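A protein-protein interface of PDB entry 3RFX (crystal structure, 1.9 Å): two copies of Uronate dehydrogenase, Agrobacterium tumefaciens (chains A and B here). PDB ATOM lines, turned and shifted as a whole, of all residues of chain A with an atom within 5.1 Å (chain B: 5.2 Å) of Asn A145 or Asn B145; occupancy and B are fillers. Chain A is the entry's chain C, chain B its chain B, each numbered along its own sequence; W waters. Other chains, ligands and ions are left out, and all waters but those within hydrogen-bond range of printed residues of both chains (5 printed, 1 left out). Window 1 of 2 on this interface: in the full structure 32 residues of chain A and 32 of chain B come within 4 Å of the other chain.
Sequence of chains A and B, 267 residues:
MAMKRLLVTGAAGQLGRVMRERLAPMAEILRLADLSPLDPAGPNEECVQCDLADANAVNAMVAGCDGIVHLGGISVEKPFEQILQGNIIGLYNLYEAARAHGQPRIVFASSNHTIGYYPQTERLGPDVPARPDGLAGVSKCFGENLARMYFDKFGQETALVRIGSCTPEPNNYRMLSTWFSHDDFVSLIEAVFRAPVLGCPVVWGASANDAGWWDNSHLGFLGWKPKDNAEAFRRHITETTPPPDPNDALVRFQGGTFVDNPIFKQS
Pro A132 touches Asn B145, and with the chains exchanged Asn A145 touches Pro B132.
Pro A132 touches Met B149, and with the chains exchanged Met A149 touches Pro B132.
Val A138 touches Met B149, and with the chains exchanged Met A149 touches Val B138.
Cys A141 touches Asn B145, and with the chains exchanged Asn A145 touches Cys B141.
Of the 18 pairs that touch across the chains among the printed residues, 17 have their exchanged pair printed and touching as well.
Asn A145 touches just these residues of chain B: Ala B130 (3.9 Å), Pro B132 (3.8 Å), Val B138 (3.8 Å), Cys B141 (3.3 Å) and Asn B145 (3.3 Å).
Asn B145 touches just these residues of chain A: Ala A130, Pro A132, Val A138, Cys A141 and Asn A145.
Of the printed residues of chain A, Leu B146 touches Val A138 (3.97 Å).
Of the printed residues of chain B, Cys A141 touches Asn B145.
Of the printed residues of chain A, Arg B148 touches Ala A130 (3.9 Å).
Printed residues of chain B within 4 Å of Ala A130: Asn B145 and Arg B148.
Of the printed residues of chain B, Phe A142 touches Val B138.
The nearest residue of chain B that does not touch Asn A145 is Phe B142 (4.8 Å).
The nearest residue of chain A that does not touch Asn B145 is Phe A142 (4.8 Å).
The nearest printed residue of chain A that does not touch Leu B146 is Pro A132 (5.6 Å).
O of Cys B141 lies within hydrogen-bond range of ND2 of Asn B145 (3.3 Å).
The backbone carbonyl oxygen (O) of Cys A141 is in hydrogen-bond range of the side-chain amide nitrogen (ND2) of Asn A145, 3.2 Å away.
ND2 of Asn B145 sits close to ND2 of Asn A145, 3.3 Å away.
Water W5 lies within hydrogen-bond range of ND2 of Asn B145, O of Val A138 and N of Phe A142.
Water W4 lies within hydrogen-bond range of the side-chain amide nitrogen of Asn A145, the backbone carbonyl oxygen of Val B138 and the backbone NH of Phe B142.
Water W3 bridges O of Pro B132 (2.9 Å) and O of Arg A148 (3.4 Å).
Water W1 bridges O of Pro A132 (2.9 Å) and O of Arg B148 (3.4 Å).
Water W2 bridges OD1 of Asn B145 and O of Ala A130.
O of Ala A130 touches CG of Arg B148, 3.9 Å away.
Pro A132 touches Asn B145.
Pro A132 touches Met B149 (O to CG, 3.3 Å).
Val A138 touches Phe B142 (CG1 to CE1, 3.5 Å).
Val A138 touches Asn B145 (CG2 to O, 3.8 Å).
CB of Cys A141 touches ND2 of Asn B145 (3.3 Å).
CE1 of Phe A142 touches CG1 of Val B138, at 3.5 Å.
O of Asn A145 touches CG2 of Val B138, 3.8 Å away.
CG of Met A149 touches O of Pro B132, at 3.3 Å.
CG2 of Val B138 touches CB of Met A149, 3.9 Å away.
Of the 12 printed residues of chain A, 8 touch a printed residue of chain B.
Hydrophobic or aromatic side chains of chain A that line the printed part of chain B: Ala A130, Pro A132, Val A138, Phe A142 and Met A149.
Of the 12 printed residues of chain B, 9 touch a printed residue of chain A.
Among the printed residues, 18 pairs touch across the chains.
Among the printed residues, no Asp or Glu carboxylate lies within 4 Å of a Lys or Arg side-chain nitrogen of the other chain.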
ATOM      1  N   ALA A 130      29.794 -10.857  25.748  1.00  0.00           N
ATOM      2  CA  ALA A 130      29.712  -9.729  24.834  1.00  0.00           C
ATOM      3  C   ALA A 130      30.966  -8.856  24.910  1.00  0.00           C
ATOM      4  O   ALA A 130      31.538  -8.671  25.980  1.00  0.00           O
ATOM      5  CB  ALA A 130      28.472  -8.891  25.149  1.00  0.00           C
ATOM      6  N   PRO A 132      31.031  -5.414  23.063  1.00  0.00           N
ATOM      7  CA  PRO A 132      30.426  -4.447  22.134  1.00  0.00           C
ATOM      8  C   PRO A 132      31.419  -3.378  21.697  1.00  0.00           C
ATOM      9  O   PRO A 132      32.239  -2.936  22.504  1.00  0.00           O
ATOM     10  CB  PRO A 132      29.310  -3.786  22.968  1.00  0.00           C
ATOM     11  CG  PRO A 132      29.131  -4.636  24.168  1.00  0.00           C
ATOM     12  CD  PRO A 132      30.425  -5.365  24.404  1.00  0.00           C
ATOM     13  N   VAL A 138      26.263  -1.996  22.363  1.00  0.00           N
ATOM     14  CA  VAL A 138      25.754  -2.135  23.734  1.00  0.00           C
ATOM     15  C   VAL A 138      24.221  -2.189  23.718  1.00  0.00           C
ATOM     16  O   VAL A 138      23.602  -2.961  24.454  1.00  0.00           O
ATOM     17  CB  VAL A 138      26.262  -0.991  24.665  1.00  0.00           C
ATOM     18  CG1 VAL A 138      25.523  -0.995  26.018  1.00  0.00           C
ATOM     19  CG2 VAL A 138      27.776  -1.104  24.887  1.00  0.00           C
ATOM     20  N   CYS A 141      22.950  -5.557  22.635  1.00  0.00           N
ATOM     21  CA  CYS A 141      23.041  -6.435  23.807  1.00  0.00           C
ATOM     22  C   CYS A 141      21.835  -6.237  24.713  1.00  0.00           C
ATOM     23  O   CYS A 141      21.301  -7.191  25.271  1.00  0.00           O
ATOM     24  CB  CYS A 141      24.297  -6.149  24.622  1.00  0.00           C
ATOM     25  SG  CYS A 141      25.852  -6.626  23.815  1.00  0.00           S
ATOM     26  N   PHE A 142      21.409  -4.988  24.875  1.00  0.00           N
ATOM     27  CA  PHE A 142      20.235  -4.726  25.705  1.00  0.00           C
ATOM     28  C   PHE A 142      19.035  -5.484  25.150  1.00  0.00           C
ATOM     29  O   PHE A 142      18.285  -6.115  25.903  1.00  0.00           O
ATOM     30  CB  PHE A 142      19.930  -3.227  25.766  1.00  0.00           C
ATOM     31  CG  PHE A 142      18.622  -2.908  26.434  1.00  0.00           C
ATOM     32  CD1 PHE A 142      18.545  -2.798  27.816  1.00  0.00           C
ATOM     33  CD2 PHE A 142      17.468  -2.740  25.682  1.00  0.00           C
ATOM     34  CE1 PHE A 142      17.335  -2.514  28.445  1.00  0.00           C
ATOM     35  CE2 PHE A 142      16.247  -2.452  26.301  1.00  0.00           C
ATOM     36  CZ  PHE A 142      16.184  -2.346  27.689  1.00  0.00           C
ATOM     37  N   GLY A 143      18.836  -5.397  23.835  1.00  0.00           N
ATOM     38  CA  GLY A 143      17.756  -6.127  23.187  1.00  0.00           C
ATOM     39  C   GLY A 143      17.829  -7.627  23.448  1.00  0.00           C
ATOM     40  O   GLY A 143      16.813  -8.271  23.739  1.00  0.00           O
ATOM     41  N   GLU A 144      19.022  -8.200  23.328  1.00  0.00           N
ATOM     42  CA  GLU A 144      19.198  -9.633  23.617  1.00  0.00           C
ATOM     43  C   GLU A 144      18.870  -9.982  25.069  1.00  0.00           C
ATOM     44  O   GLU A 144      18.251 -11.012  25.338  1.00  0.00           O
ATOM     45  CB  GLU A 144      20.635 -10.083  23.304  1.00  0.00           C
ATOM     46  CG  GLU A 144      21.019  -9.936  21.838  1.00  0.00           C
ATOM     47  CD  GLU A 144      22.386 -10.545  21.525  1.00  0.00           C
ATOM     48  OE1 GLU A 144      23.028 -11.097  22.450  1.00  0.00           O
ATOM     49  OE2 GLU A 144      22.812 -10.471  20.350  1.00  0.00           O
ATOM     50  N   ASN A 145      19.320  -9.151  26.007  1.00  0.00           N
ATOM     51  CA  ASN A 145      19.102  -9.443  27.422  1.00  0.00           C
ATOM     52  C   ASN A 145      17.626  -9.301  27.780  1.00  0.00           C
ATOM     53  O   ASN A 145      17.074 -10.099  28.544  1.00  0.00           O
ATOM     54  CB  ASN A 145      19.954  -8.531  28.309  1.00  0.00           C
ATOM     55  CG  ASN A 145      21.449  -8.798  28.155  1.00  0.00           C
ATOM     56  OD1 ASN A 145      21.868  -9.935  27.896  1.00  0.00           O
ATOM     57  ND2 ASN A 145      22.256  -7.756  28.323  1.00  0.00           N
ATOM     58  N   LEU A 146      16.998  -8.271  27.227  1.00  0.00           N
ATOM     59  CA  LEU A 146      15.569  -8.061  27.433  1.00  0.00           C
ATOM     60  C   LEU A 146      14.771  -9.230  26.853  1.00  0.00           C
ATOM     61  O   LEU A 146      13.874  -9.771  27.502  1.00  0.00           O
ATOM     62  CB  LEU A 146      15.127  -6.748  26.776  1.00  0.00           C
ATOM     63  CG  LEU A 146      13.696  -6.346  27.147  1.00  0.00           C
ATOM     64  CD1 LEU A 146      13.682  -5.757  28.543  1.00  0.00           C
ATOM     65  CD2 LEU A 146      13.142  -5.341  26.146  1.00  0.00           C
ATOM     66  N   ALA A 147      15.108  -9.638  25.632  1.00  0.00           N
ATOM     67  CA  ALA A 147      14.415 -10.762  25.012  1.00  0.00           C
ATOM     68  C   ALA A 147      14.537 -12.021  25.869  1.00  0.00           C
ATOM     69  O   ALA A 147      13.577 -12.777  26.029  1.00  0.00           O
ATOM     70  CB  ALA A 147      14.970 -11.022  23.601  1.00  0.00           C
ATOM     71  N   ARG A 148      15.729 -12.257  26.404  1.00  0.00           N
ATOM     72  CA  ARG A 148      15.940 -13.460  27.205  1.00  0.00           C
ATOM     73  C   ARG A 148      15.081 -13.420  28.472  1.00  0.00           C
ATOM     74  O   ARG A 148      14.494 -14.426  28.869  1.00  0.00           O
ATOM     75  CB  ARG A 148      17.426 -13.625  27.553  1.00  0.00           C
ATOM     76  CG  ARG A 148      17.717 -14.849  28.410  1.00  0.00           C
ATOM     77  CD  ARG A 148      17.526 -16.137  27.617  1.00  0.00           C
ATOM     78  NE  ARG A 148      17.116 -17.238  28.487  1.00  0.00           N
ATOM     79  CZ  ARG A 148      17.246 -18.520  28.170  1.00  0.00           C
ATOM     80  NH1 ARG A 148      17.802 -18.852  27.014  1.00  0.00           N
ATOM     81  NH2 ARG A 148      16.822 -19.464  29.005  1.00  0.00           N
ATOM     82  N   MET A 149      15.008 -12.255  29.105  1.00  0.00           N
ATOM     83  CA  MET A 149      14.157 -12.099  30.285  1.00  0.00           C
ATOM     84  C   MET A 149      12.682 -12.393  29.968  1.00  0.00           C
ATOM     85  O   MET A 149      12.016 -13.111  30.720  1.00  0.00           O
ATOM     86  CB  MET A 149      14.326 -10.700  30.904  1.00  0.00           C
ATOM     87  CG  MET A 149      13.617 -10.528  32.239  1.00  0.00           C
ATOM     88  SD  MET A 149      11.908  -9.946  32.027  1.00  0.00           S
ATOM     89  CE  MET A 149      12.270  -8.262  31.536  1.00  0.00           C
ATOM     90  N   ALA B 130      23.994 -14.254  30.361  1.00  0.00           N
ATOM     91  CA  ALA B 130      23.029 -13.601  31.251  1.00  0.00           C
ATOM     92  C   ALA B 130      21.664 -14.275  31.192  1.00  0.00           C
ATOM     93  O   ALA B 130      21.220 -14.704  30.133  1.00  0.00           O
ATOM     94  CB  ALA B 130      22.897 -12.102  30.915  1.00  0.00           C
ATOM     95  N   PRO B 132      18.658 -12.600  33.020  1.00  0.00           N
ATOM     96  CA  PRO B 132      18.150 -11.613  33.989  1.00  0.00           C
ATOM     97  C   PRO B 132      16.719 -11.940  34.413  1.00  0.00           C
ATOM     98  O   PRO B 132      15.942 -12.447  33.609  1.00  0.00           O
ATOM     99  CB  PRO B 132      18.190 -10.280  33.214  1.00  0.00           C
ATOM    100  CG  PRO B 132      18.874 -10.563  31.904  1.00  0.00           C
ATOM    101  CD  PRO B 132      18.810 -12.040  31.663  1.00  0.00           C
ATOM    102  N   VAL B 138      18.102  -6.749  33.801  1.00  0.00           N
ATOM    103  CA  VAL B 138      18.455  -6.363  32.438  1.00  0.00           C
ATOM    104  C   VAL B 138      19.261  -5.070  32.451  1.00  0.00           C
ATOM    105  O   VAL B 138      20.224  -4.926  31.700  1.00  0.00           O
ATOM    106  CB  VAL B 138      17.188  -6.205  31.538  1.00  0.00           C
ATOM    107  CG1 VAL B 138      17.530  -5.528  30.197  1.00  0.00           C
ATOM    108  CG2 VAL B 138      16.534  -7.568  31.307  1.00  0.00           C
ATOM    109  N   CYS B 141      22.809  -5.681  33.533  1.00  0.00           N
ATOM    110  CA  CYS B 141      23.536  -6.194  32.369  1.00  0.00           C
ATOM    111  C   CYS B 141      23.972  -5.042  31.472  1.00  0.00           C
ATOM    112  O   CYS B 141      25.070  -5.055  30.931  1.00  0.00           O
ATOM    113  CB  CYS B 141      22.675  -7.154  31.542  1.00  0.00           C
ATOM    114  SG  CYS B 141      22.360  -8.741  32.330  1.00  0.00           S
ATOM    115  N   PHE B 142      23.097  -4.052  31.296  1.00  0.00           N
ATOM    116  CA  PHE B 142      23.453  -2.892  30.476  1.00  0.00           C
ATOM    117  C   PHE B 142      24.703  -2.219  31.021  1.00  0.00           C
ATOM    118  O   PHE B 142      25.623  -1.881  30.271  1.00  0.00           O
ATOM    119  CB  PHE B 142      22.298  -1.876  30.399  1.00  0.00           C
ATOM    120  CG  PHE B 142      22.677  -0.594  29.699  1.00  0.00           C
ATOM    121  CD1 PHE B 142      22.514  -0.468  28.328  1.00  0.00           C
ATOM    122  CD2 PHE B 142      23.214   0.469  30.409  1.00  0.00           C
ATOM    123  CE1 PHE B 142      22.880   0.699  27.672  1.00  0.00           C
ATOM    124  CE2 PHE B 142      23.587   1.645  29.768  1.00  0.00           C
ATOM    125  CZ  PHE B 142      23.418   1.763  28.398  1.00  0.00           C
ATOM    126  N   GLY B 143      24.736  -2.018  32.335  1.00  0.00           N
ATOM    127  CA  GLY B 143      25.920  -1.462  32.967  1.00  0.00           C
ATOM    128  C   GLY B 143      27.169  -2.292  32.696  1.00  0.00           C
ATOM    129  O   GLY B 143      28.246  -1.745  32.428  1.00  0.00           O
ATOM    130  N   GLU B 144      27.044  -3.614  32.779  1.00  0.00           N
ATOM    131  CA  GLU B 144      28.202  -4.483  32.516  1.00  0.00           C
ATOM    132  C   GLU B 144      28.670  -4.368  31.055  1.00  0.00           C
ATOM    133  O   GLU B 144      29.869  -4.281  30.781  1.00  0.00           O
ATOM    134  CB  GLU B 144      27.885  -5.949  32.848  1.00  0.00           C
ATOM    135  CG  GLU B 144      27.586  -6.231  34.335  1.00  0.00           C
ATOM    136  CD  GLU B 144      27.400  -7.725  34.617  1.00  0.00           C
ATOM    137  OE1 GLU B 144      27.543  -8.533  33.673  1.00  0.00           O
ATOM    138  OE2 GLU B 144      27.112  -8.097  35.775  1.00  0.00           O
ATOM    139  N   ASN B 145      27.725  -4.378  30.117  1.00  0.00           N
ATOM    140  CA  ASN B 145      28.085  -4.282  28.707  1.00  0.00           C
ATOM    141  C   ASN B 145      28.704  -2.931  28.358  1.00  0.00           C
ATOM    142  O   ASN B 145      29.677  -2.865  27.598  1.00  0.00           O
ATOM    143  CB  ASN B 145      26.882  -4.571  27.809  1.00  0.00           C
ATOM    144  CG  ASN B 145      26.344  -5.981  27.989  1.00  0.00           C
ATOM    145  OD1 ASN B 145      27.100  -6.918  28.265  1.00  0.00           O
ATOM    146  ND2 ASN B 145      25.038  -6.140  27.823  1.00  0.00           N
ATOM    147  N   LEU B 146      28.141  -1.855  28.910  1.00  0.00           N
ATOM    148  CA  LEU B 146      28.690  -0.516  28.703  1.00  0.00           C
ATOM    149  C   LEU B 146      30.106  -0.417  29.270  1.00  0.00           C
ATOM    150  O   LEU B 146      31.007   0.106  28.616  1.00  0.00           O
ATOM    151  CB  LEU B 146      27.802   0.547  29.365  1.00  0.00           C
ATOM    152  CG  LEU B 146      28.147   2.007  29.018  1.00  0.00           C
ATOM    153  CD1 LEU B 146      27.645   2.359  27.625  1.00  0.00           C
ATOM    154  CD2 LEU B 146      27.566   2.969  30.035  1.00  0.00           C
ATOM    155  N   ALA B 147      30.296  -0.904  30.493  1.00  0.00           N
ATOM    156  CA  ALA B 147      31.618  -0.854  31.136  1.00  0.00           C
ATOM    157  C   ALA B 147      32.662  -1.590  30.301  1.00  0.00           C
ATOM    158  O   ALA B 147      33.784  -1.105  30.138  1.00  0.00           O
ATOM    159  CB  ALA B 147      31.573  -1.423  32.562  1.00  0.00           C
ATOM    160  N   ARG B 148      32.293  -2.760  29.781  1.00  0.00           N
ATOM    161  CA  ARG B 148      33.203  -3.542  28.936  1.00  0.00           C
ATOM    162  C   ARG B 148      33.595  -2.753  27.692  1.00  0.00           C
ATOM    163  O   ARG B 148      34.752  -2.760  27.276  1.00  0.00           O
ATOM    164  CB  ARG B 148      32.554  -4.877  28.522  1.00  0.00           C
ATOM    165  CG  ARG B 148      33.473  -5.788  27.685  1.00  0.00           C
ATOM    166  CD  ARG B 148      34.671  -6.321  28.503  1.00  0.00           C
ATOM    167  NE  ARG B 148      35.880  -6.456  27.680  1.00  0.00           N
ATOM    168  CZ  ARG B 148      36.949  -7.185  27.997  1.00  0.00           C
ATOM    169  NH1 ARG B 148      36.970  -7.888  29.121  1.00  0.00           N
ATOM    170  NH2 ARG B 148      37.999  -7.214  27.178  1.00  0.00           N
ATOM    171  N   MET B 149      32.622  -2.074  27.090  1.00  0.00           N
ATOM    172  CA  MET B 149      32.891  -1.285  25.894  1.00  0.00           C
ATOM    173  C   MET B 149      33.852  -0.145  26.193  1.00  0.00           C
ATOM    174  O   MET B 149      34.783   0.095  25.417  1.00  0.00           O
ATOM    175  CB  MET B 149      31.587  -0.740  25.286  1.00  0.00           C
ATOM    176  CG  MET B 149      31.791  -0.031  23.935  1.00  0.00           C
ATOM    177  SD  MET B 149      32.117   1.742  24.120  1.00  0.00           S
ATOM    178  CE  MET B 149      30.464   2.318  24.538  1.00  0.00           C
HETATM  179  O   HOH W   1      33.584  -4.465  24.554  1.00  0.00           O
HETATM  180  O   HOH W   2      29.950  -7.395  28.191  1.00  0.00           O
HETATM  181  O   HOH W   3      16.534 -14.374  31.590  1.00  0.00           O
HETATM  182  O   HOH W   4      21.200  -5.203  28.846  1.00  0.00           O
HETATM  183  O   HOH W   5      23.365  -3.946  27.343  1.00  0.00           O
